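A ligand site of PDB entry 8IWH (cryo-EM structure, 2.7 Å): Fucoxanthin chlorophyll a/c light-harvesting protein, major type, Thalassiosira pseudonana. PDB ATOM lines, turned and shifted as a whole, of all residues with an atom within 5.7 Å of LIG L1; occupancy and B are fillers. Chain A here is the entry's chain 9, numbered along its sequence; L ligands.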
ATOM      1  N   ILE A  38      25.597   1.016  11.398  1.00  0.00           N
ATOM      2  CA  ILE A  38      24.988   1.999  12.288  1.00  0.00           C
ATOM      3  C   ILE A  38      25.873   2.207  13.513  1.00  0.00           C
ATOM      4  O   ILE A  38      26.447   3.286  13.689  1.00  0.00           O
ATOM      5  CB  ILE A  38      23.572   1.573  12.698  1.00  0.00           C
ATOM      6  N   ALA A  39      25.999   1.167  14.345  1.00  0.00           N
ATOM      7  CA  ALA A  39      26.738   1.221  15.609  1.00  0.00           C
ATOM      8  C   ALA A  39      26.677  -0.096  16.383  1.00  0.00           C
ATOM      9  O   ALA A  39      27.731  -0.678  16.653  1.00  0.00           O
ATOM     10  CB  ALA A  39      26.237   2.363  16.502  1.00  0.00           C
ATOM     11  N   PRO A  40      25.488  -0.587  16.757  1.00  0.00           N
ATOM     12  CA  PRO A  40      25.452  -1.717  17.706  1.00  0.00           C
ATOM     13  C   PRO A  40      26.152  -2.969  17.205  1.00  0.00           C
ATOM     14  O   PRO A  40      26.721  -3.715  18.007  1.00  0.00           O
ATOM     15  CB  PRO A  40      23.952  -1.961  17.915  1.00  0.00           C
ATOM     16  CG  PRO A  40      23.268  -0.747  17.376  1.00  0.00           C
ATOM     17  CD  PRO A  40      24.135  -0.288  16.259  1.00  0.00           C
ATOM     18  N   GLU A 147      22.331  10.342   7.647  1.00  0.00           N
ATOM     19  CA  GLU A 147      21.652   9.755   8.787  1.00  0.00           C
ATOM     20  C   GLU A 147      20.185   9.466   8.484  1.00  0.00           C
ATOM     21  O   GLU A 147      19.619   8.513   9.028  1.00  0.00           O
ATOM     22  CB  GLU A 147      21.783  10.662  10.019  1.00  0.00           C
ATOM     23  CG  GLU A 147      21.244  12.069   9.845  1.00  0.00           C
ATOM     24  CD  GLU A 147      21.646  12.971  10.991  1.00  0.00           C
ATOM     25  OE1 GLU A 147      22.456  12.546  11.839  1.00  0.00           O
ATOM     26  OE2 GLU A 147      21.151  14.123  11.056  1.00  0.00           O
ATOM     27  N   LEU A 150      20.281   6.240   6.795  1.00  0.00           N
ATOM     28  CA  LEU A 150      20.496   5.208   7.800  1.00  0.00           C
ATOM     29  C   LEU A 150      19.205   4.872   8.542  1.00  0.00           C
ATOM     30  O   LEU A 150      18.910   3.705   8.782  1.00  0.00           O
ATOM     31  CB  LEU A 150      21.577   5.661   8.787  1.00  0.00           C
ATOM     32  CG  LEU A 150      23.027   5.506   8.322  1.00  0.00           C
ATOM     33  CD1 LEU A 150      23.976   5.810   9.477  1.00  0.00           C
ATOM     34  CD2 LEU A 150      23.280   4.119   7.772  1.00  0.00           C
ATOM     35  N   GLN A 151      18.432   5.900   8.908  1.00  0.00           N
ATOM     36  CA  GLN A 151      17.162   5.666   9.573  1.00  0.00           C
ATOM     37  C   GLN A 151      16.199   4.898   8.671  1.00  0.00           C
ATOM     38  O   GLN A 151      15.512   3.975   9.128  1.00  0.00           O
ATOM     39  CB  GLN A 151      16.536   7.002   9.975  1.00  0.00           C
ATOM     40  CG  GLN A 151      17.266   7.751  11.072  1.00  0.00           C
ATOM     41  CD  GLN A 151      16.697   9.126  11.308  1.00  0.00           C
ATOM     42  OE1 GLN A 151      15.783   9.556  10.603  1.00  0.00           O
ATOM     43  NE2 GLN A 151      17.235   9.831  12.295  1.00  0.00           N
ATOM     44  N   GLU A 152      16.143   5.276   7.398  1.00  0.00           N
ATOM     45  CA  GLU A 152      15.280   4.563   6.457  1.00  0.00           C
ATOM     46  C   GLU A 152      15.670   3.098   6.363  1.00  0.00           C
ATOM     47  O   GLU A 152      14.812   2.209   6.403  1.00  0.00           O
ATOM     48  CB  GLU A 152      15.356   5.217   5.076  1.00  0.00           C
ATOM     49  CG  GLU A 152      14.273   4.781   4.116  1.00  0.00           C
ATOM     50  CD  GLU A 152      14.243   5.606   2.857  1.00  0.00           C
ATOM     51  OE1 GLU A 152      15.307   6.130   2.469  1.00  0.00           O
ATOM     52  OE2 GLU A 152      13.164   5.745   2.247  1.00  0.00           O
ATOM     53  N   GLN A 154      17.325   1.268   8.653  1.00  0.00           N
ATOM     54  CA  GLN A 154      17.036   0.569   9.900  1.00  0.00           C
ATOM     55  C   GLN A 154      15.547   0.257  10.048  1.00  0.00           C
ATOM     56  O   GLN A 154      15.168  -0.848  10.452  1.00  0.00           O
ATOM     57  CB  GLN A 154      17.525   1.397  11.090  1.00  0.00           C
ATOM     58  CG  GLN A 154      19.031   1.595  11.148  1.00  0.00           C
ATOM     59  CD  GLN A 154      19.785   0.331  11.501  1.00  0.00           C
ATOM     60  OE1 GLN A 154      20.465  -0.258  10.658  1.00  0.00           O
ATOM     61  NE2 GLN A 154      19.681  -0.098  12.749  1.00  0.00           N
ATOM     62  N   HIS A 155      14.691   1.221   9.700  1.00  0.00           N
ATOM     63  CA  HIS A 155      13.250   0.974   9.743  1.00  0.00           C
ATOM     64  C   HIS A 155      12.849  -0.117   8.757  1.00  0.00           C
ATOM     65  O   HIS A 155      11.995  -0.961   9.051  1.00  0.00           O
ATOM     66  CB  HIS A 155      12.483   2.261   9.469  1.00  0.00           C
ATOM     67  CG  HIS A 155      12.707   3.322  10.495  1.00  0.00           C
ATOM     68  ND1 HIS A 155      13.323   4.522  10.211  1.00  0.00           N
ATOM     69  CD2 HIS A 155      12.396   3.369  11.817  1.00  0.00           C
ATOM     70  CE1 HIS A 155      13.379   5.263  11.302  1.00  0.00           C
ATOM     71  NE2 HIS A 155      12.830   4.585  12.284  1.00  0.00           N
ATOM     72  N   LEU A 158      13.793  -3.451  10.416  1.00  0.00           N
ATOM     73  CA  LEU A 158      12.770  -3.837  11.428  1.00  0.00           C
ATOM     74  C   LEU A 158      11.601  -4.512  10.714  1.00  0.00           C
ATOM     75  O   LEU A 158      11.297  -5.666  11.063  1.00  0.00           O
ATOM     76  CB  LEU A 158      12.300  -2.586  12.174  1.00  0.00           C
ATOM     77  CG  LEU A 158      11.805  -2.832  13.601  1.00  0.00           C
ATOM     78  CD1 LEU A 158      12.376  -4.130  14.158  1.00  0.00           C
ATOM     79  CD2 LEU A 158      12.171  -1.654  14.502  1.00  0.00           C
HETATM   80 MG1  LIG L   1      19.517   1.703  17.342  1.00  0.00          MG
HETATM   81  C1  LIG L   1      18.739   4.220  15.082  1.00  0.00           C
HETATM   82  C2  LIG L   1      22.136   3.548  18.484  1.00  0.00           C
HETATM   83  C3  LIG L   1      20.151  -0.751  19.659  1.00  0.00           C
HETATM   84  C4  LIG L   1      16.768  -0.168  16.127  1.00  0.00           C
HETATM   85  N1  LIG L   1      20.308   3.570  16.826  1.00  0.00           N
HETATM   86  C5  LIG L   1      19.831   4.473  15.861  1.00  0.00           C
HETATM   87  C6  LIG L   1      20.699   5.728  15.811  1.00  0.00           C
HETATM   88  C7  LIG L   1      21.856   5.402  16.786  1.00  0.00           C
HETATM   89  C8  LIG L   1      21.421   4.086  17.431  1.00  0.00           C
HETATM   90  C9  LIG L   1      23.171   5.268  16.063  1.00  0.00           C
HETATM   91  C10 LIG L   1      19.932   6.942  16.296  1.00  0.00           C
HETATM   92  N2  LIG L   1      20.902   1.429  18.771  1.00  0.00           N
HETATM   93  C11 LIG L   1      21.838   2.351  19.143  1.00  0.00           C
HETATM   94  C12 LIG L   1      22.547   1.877  20.375  1.00  0.00           C
HETATM   95  C13 LIG L   1      21.988   0.670  20.710  1.00  0.00           C
HETATM   96  C14 LIG L   1      20.944   0.359  19.700  1.00  0.00           C
HETATM   97  C15 LIG L   1      23.606   2.634  21.026  1.00  0.00           C
HETATM   98  C16 LIG L   1      22.311  -0.212  21.809  1.00  0.00           C
HETATM   99  C17 LIG L   1      21.444  -0.639  22.728  1.00  0.00           C
HETATM  100  N3  LIG L   1      18.648  -0.139  17.780  1.00  0.00           N
HETATM  101  C18 LIG L   1      19.083  -0.993  18.749  1.00  0.00           C
HETATM  102  C19 LIG L   1      18.258  -2.195  18.771  1.00  0.00           C
HETATM  103  C20 LIG L   1      17.284  -2.020  17.795  1.00  0.00           C
HETATM  104  C21 LIG L   1      17.531  -0.725  17.175  1.00  0.00           C
HETATM  105  C22 LIG L   1      18.447  -3.331  19.680  1.00  0.00           C
HETATM  106  C23 LIG L   1      16.219  -2.968  17.431  1.00  0.00           C
HETATM  107  C24 LIG L   1      14.907  -2.648  18.113  1.00  0.00           C
HETATM  108  N4  LIG L   1      18.081   1.892  15.927  1.00  0.00           N
HETATM  109  C25 LIG L   1      17.012   1.051  15.532  1.00  0.00           C
HETATM  110  C26 LIG L   1      16.253   1.719  14.451  1.00  0.00           C
HETATM  111  C27 LIG L   1      16.872   2.935  14.243  1.00  0.00           C
HETATM  112  C28 LIG L   1      18.002   2.999  15.181  1.00  0.00           C
HETATM  113  C29 LIG L   1      15.079   1.140  13.797  1.00  0.00           C
HETATM  114  C30 LIG L   1      16.875   4.172  13.476  1.00  0.00           C
HETATM  115  O1  LIG L   1      16.113   4.540  12.587  1.00  0.00           O
HETATM  116  C31 LIG L   1      18.063   5.029  13.999  1.00  0.00           C
HETATM  117  C32 LIG L   1      19.033   5.397  12.905  1.00  0.00           C
HETATM  118  O2  LIG L   1      19.403   4.700  11.959  1.00  0.00           O
HETATM  119  O3  LIG L   1      19.535   6.652  13.019  1.00  0.00           O
HETATM  120  C33 LIG L   1      20.662   6.998  12.210  1.00  0.00           C
HETATM  121  C1  LG2 L   2      14.913 -19.316  14.948  1.00  0.00           C
HETATM  122  O1  LG2 L   2      16.937  -6.213  16.175  1.00  0.00           O
HETATM  123  C2  LG2 L   2      13.724 -18.893  15.754  1.00  0.00           C
HETATM  124  C3  LG2 L   2      16.681  -9.599  15.728  1.00  0.00           C
HETATM  125  C4  LG2 L   2      16.185  -8.352  15.714  1.00  0.00           C
HETATM  126  C5  LG2 L   2      14.733  -8.124  15.979  1.00  0.00           C
HETATM  127  C6  LG2 L   2      17.036  -7.198  15.454  1.00  0.00           C
HETATM  128  C7  LG2 L   2      18.032  -7.202  14.313  1.00  0.00           C
HETATM  129  C8  LG2 L   2      18.704  -5.846  14.204  1.00  0.00           C
HETATM  130  C9  LG2 L   2      19.968  -5.494  14.987  1.00  0.00           C
HETATM  131  C10 LG2 L   2      19.830  -4.095  15.571  1.00  0.00           C
HETATM  132  C11 LG2 L   2      19.698  -3.141  14.406  1.00  0.00           C
HETATM  133  C12 LG2 L   2      18.306  -3.270  13.818  1.00  0.00           C
HETATM  134  C13 LG2 L   2      13.558 -17.619  16.121  1.00  0.00           C
HETATM  135  C14 LG2 L   2      17.859  -4.720  13.604  1.00  0.00           C
HETATM  136  C15 LG2 L   2      16.497  -4.845  12.929  1.00  0.00           C
HETATM  137  C16 LG2 L   2      21.171  -5.533  14.071  1.00  0.00           C
HETATM  138  C17 LG2 L   2      20.179  -6.491  16.125  1.00  0.00           C
HETATM  139  C18 LG2 L   2      12.749 -19.928  16.172  1.00  0.00           C
HETATM  140  C19 LG2 L   2      13.142 -21.205  16.227  1.00  0.00           C
HETATM  141  C20 LG2 L   2      12.221 -22.263  16.647  1.00  0.00           C
HETATM  142  C21 LG2 L   2      12.574 -23.570  16.672  1.00  0.00           C
HETATM  143  C22 LG2 L   2      13.946 -23.971  16.240  1.00  0.00           C
HETATM  144  C23 LG2 L   2      11.615 -24.607  17.132  1.00  0.00           C
HETATM  145  C24 LG2 L   2      14.532 -16.582  15.746  1.00  0.00           C
HETATM  146  C25 LG2 L   2      11.746 -25.830  16.834  1.00  0.00           C
HETATM  147  C26 LG2 L   2      11.846 -27.026  16.491  1.00  0.00           C
HETATM  148  C27 LG2 L   2      12.663 -27.969  17.327  1.00  0.00           C
HETATM  149  C28 LG2 L   2      12.239 -29.416  17.153  1.00  0.00           C
HETATM  150  C29 LG2 L   2      11.909 -29.794  15.708  1.00  0.00           C
HETATM  151  C30 LG2 L   2      10.782 -28.918  15.187  1.00  0.00           C
HETATM  152  C31 LG2 L   2      11.114 -27.434  15.231  1.00  0.00           C
HETATM  153  C32 LG2 L   2      11.931 -27.000  14.025  1.00  0.00           C
HETATM  154  C33 LG2 L   2      13.867 -30.926  14.960  1.00  0.00           C
HETATM  155  C34 LG2 L   2      13.563 -32.072  14.049  1.00  0.00           C
HETATM  156  C35 LG2 L   2      14.219 -15.295  15.844  1.00  0.00           C
HETATM  157  C36 LG2 L   2      14.143 -27.786  16.974  1.00  0.00           C
HETATM  158  C37 LG2 L   2      12.449 -27.581  18.783  1.00  0.00           C
HETATM  159  C38 LG2 L   2      15.212 -14.277  15.485  1.00  0.00           C
HETATM  160  C39 LG2 L   2      15.061 -13.012  15.917  1.00  0.00           C
HETATM  161  C40 LG2 L   2      13.857 -12.658  16.733  1.00  0.00           C
HETATM  162  C41 LG2 L   2      16.040 -11.958  15.590  1.00  0.00           C
HETATM  163  C42 LG2 L   2      15.774 -10.722  15.991  1.00  0.00           C
HETATM  164  O2  LG2 L   2      18.833  -5.437  12.845  1.00  0.00           O
HETATM  165  O3  LG2 L   2      19.925  -1.799  14.861  1.00  0.00           O
HETATM  166  O4  LG2 L   2       9.875 -26.706  15.205  1.00  0.00           O
HETATM  167  O5  LG2 L   2      13.054 -29.720  14.874  1.00  0.00           O
HETATM  168  O6  LG2 L   2      14.773 -30.956  15.784  1.00  0.00           O
HETATM  169 MG1  LG3 L   3      10.703   5.801  14.112  1.00  0.00          MG
HETATM  170  C1  LG3 L   3      13.174   8.250  14.029  1.00  0.00           C
HETATM  171  C2  LG3 L   3       8.723   7.752  12.150  1.00  0.00           C
HETATM  172  C3  LG3 L   3       8.340   3.308  14.133  1.00  0.00           C
HETATM  173  C4  LG3 L   3      12.816   3.809  16.131  1.00  0.00           C
HETATM  174  N1  LG3 L   3      10.932   7.703  13.265  1.00  0.00           N
HETATM  175  C5  LG3 L   3      12.037   8.556  13.341  1.00  0.00           C
HETATM  176  C6  LG3 L   3      11.790   9.854  12.570  1.00  0.00           C
HETATM  177  C7  LG3 L   3      10.329   9.705  12.073  1.00  0.00           C
HETATM  178  C8  LG3 L   3       9.941   8.290  12.518  1.00  0.00           C
HETATM  179  C9  LG3 L   3       9.423  10.751  12.666  1.00  0.00           C
HETATM  180  C10 LG3 L   3      12.731   9.989  11.385  1.00  0.00           C
HETATM  181  C11 LG3 L   3      12.585  11.330  10.704  1.00  0.00           C
HETATM  182  C12 LG3 L   3      13.683  12.248  11.150  1.00  0.00           C
HETATM  183  O1  LG3 L   3      14.725  11.962  11.740  1.00  0.00           O
HETATM  184  O2  LG3 L   3      13.454  13.560  10.836  1.00  0.00           O
HETATM  185  N2  LG3 L   3       8.880   5.574  13.295  1.00  0.00           N
HETATM  186  C13 LG3 L   3       8.251   6.477  12.505  1.00  0.00           C
HETATM  187  C14 LG3 L   3       6.946   5.915  12.049  1.00  0.00           C
HETATM  188  C15 LG3 L   3       6.833   4.661  12.598  1.00  0.00           C
HETATM  189  C16 LG3 L   3       8.063   4.429  13.414  1.00  0.00           C
HETATM  190  C17 LG3 L   3       6.017   6.652  11.183  1.00  0.00           C
HETATM  191  C18 LG3 L   3       5.778   3.686  12.510  1.00  0.00           C
HETATM  192  C19 LG3 L   3       4.477   3.939  12.682  1.00  0.00           C
HETATM  193  N3  LG3 L   3      10.598   3.917  14.990  1.00  0.00           N
HETATM  194  C20 LG3 L   3       9.528   3.067  14.877  1.00  0.00           C
HETATM  195  C21 LG3 L   3       9.782   1.839  15.617  1.00  0.00           C
HETATM  196  C22 LG3 L   3      11.049   1.975  16.175  1.00  0.00           C
HETATM  197  C23 LG3 L   3      11.561   3.282  15.783  1.00  0.00           C
HETATM  198  C24 LG3 L   3       8.864   0.710  15.722  1.00  0.00           C
HETATM  199  C25 LG3 L   3      11.756   0.992  17.012  1.00  0.00           C
HETATM  200  C26 LG3 L   3      11.332   1.085  18.454  1.00  0.00           C
HETATM  201  N4  LG3 L   3      12.525   5.954  14.967  1.00  0.00           N
HETATM  202  C27 LG3 L   3      13.280   5.051  15.763  1.00  0.00           C
HETATM  203  C28 LG3 L   3      14.593   5.665  16.081  1.00  0.00           C
HETATM  204  C29 LG3 L   3      14.605   6.894  15.439  1.00  0.00           C
HETATM  205  C30 LG3 L   3      13.305   7.014  14.756  1.00  0.00           C
HETATM  206  C31 LG3 L   3      15.631   5.039  16.895  1.00  0.00           C
HETATM  207  C32 LG3 L   3      15.355   8.108  15.177  1.00  0.00           C
HETATM  208  O3  LG3 L   3      16.460   8.437  15.583  1.00  0.00           O
HETATM  209  C33 LG3 L   3      14.482   8.986  14.233  1.00  0.00           C
HETATM  210  C34 LG3 L   3      14.275  10.378  14.780  1.00  0.00           C
HETATM  211  O4  LG3 L   3      15.059  11.326  14.704  1.00  0.00           O
HETATM  212  O5  LG3 L   3      13.087  10.555  15.412  1.00  0.00           O
HETATM  213  C35 LG3 L   3      13.108  11.212  16.683  1.00  0.00           C
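A ring nitrogen (NE2) of His 155 sits close to an oxygen (O1) of LIG L1, at 3.3 Å.
The backbone NH (N) of Gln 151 lies close to an oxygen (O2) of LIG L1 (3.4 Å).
O3 of LG2 L2 is in hydrogen-bond range of NE2 of Gln 154 (2.7 Å).
OE1 of Gln 151 lies close to O1 of LG3 L3 (2.9 Å).
A ring nitrogen (ND1) of His 155 sits at hydrogen-bond distance from the backbone carbonyl oxygen (O) of Gln 151.
O of Leu 150 sits close to O2 of LIG L1 (3.4 Å).
CG of Pro 40 touches C14 of LIG L1, at 3.5 Å.
O of Glu 147 touches C33 of LIG L1 (3.7 Å).
Gln 154 touches LIG L1.
Within 4 Å of LIG L1: Pro 40, Glu 147, Leu 150, Gln 151, Gln 154 and His 155.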
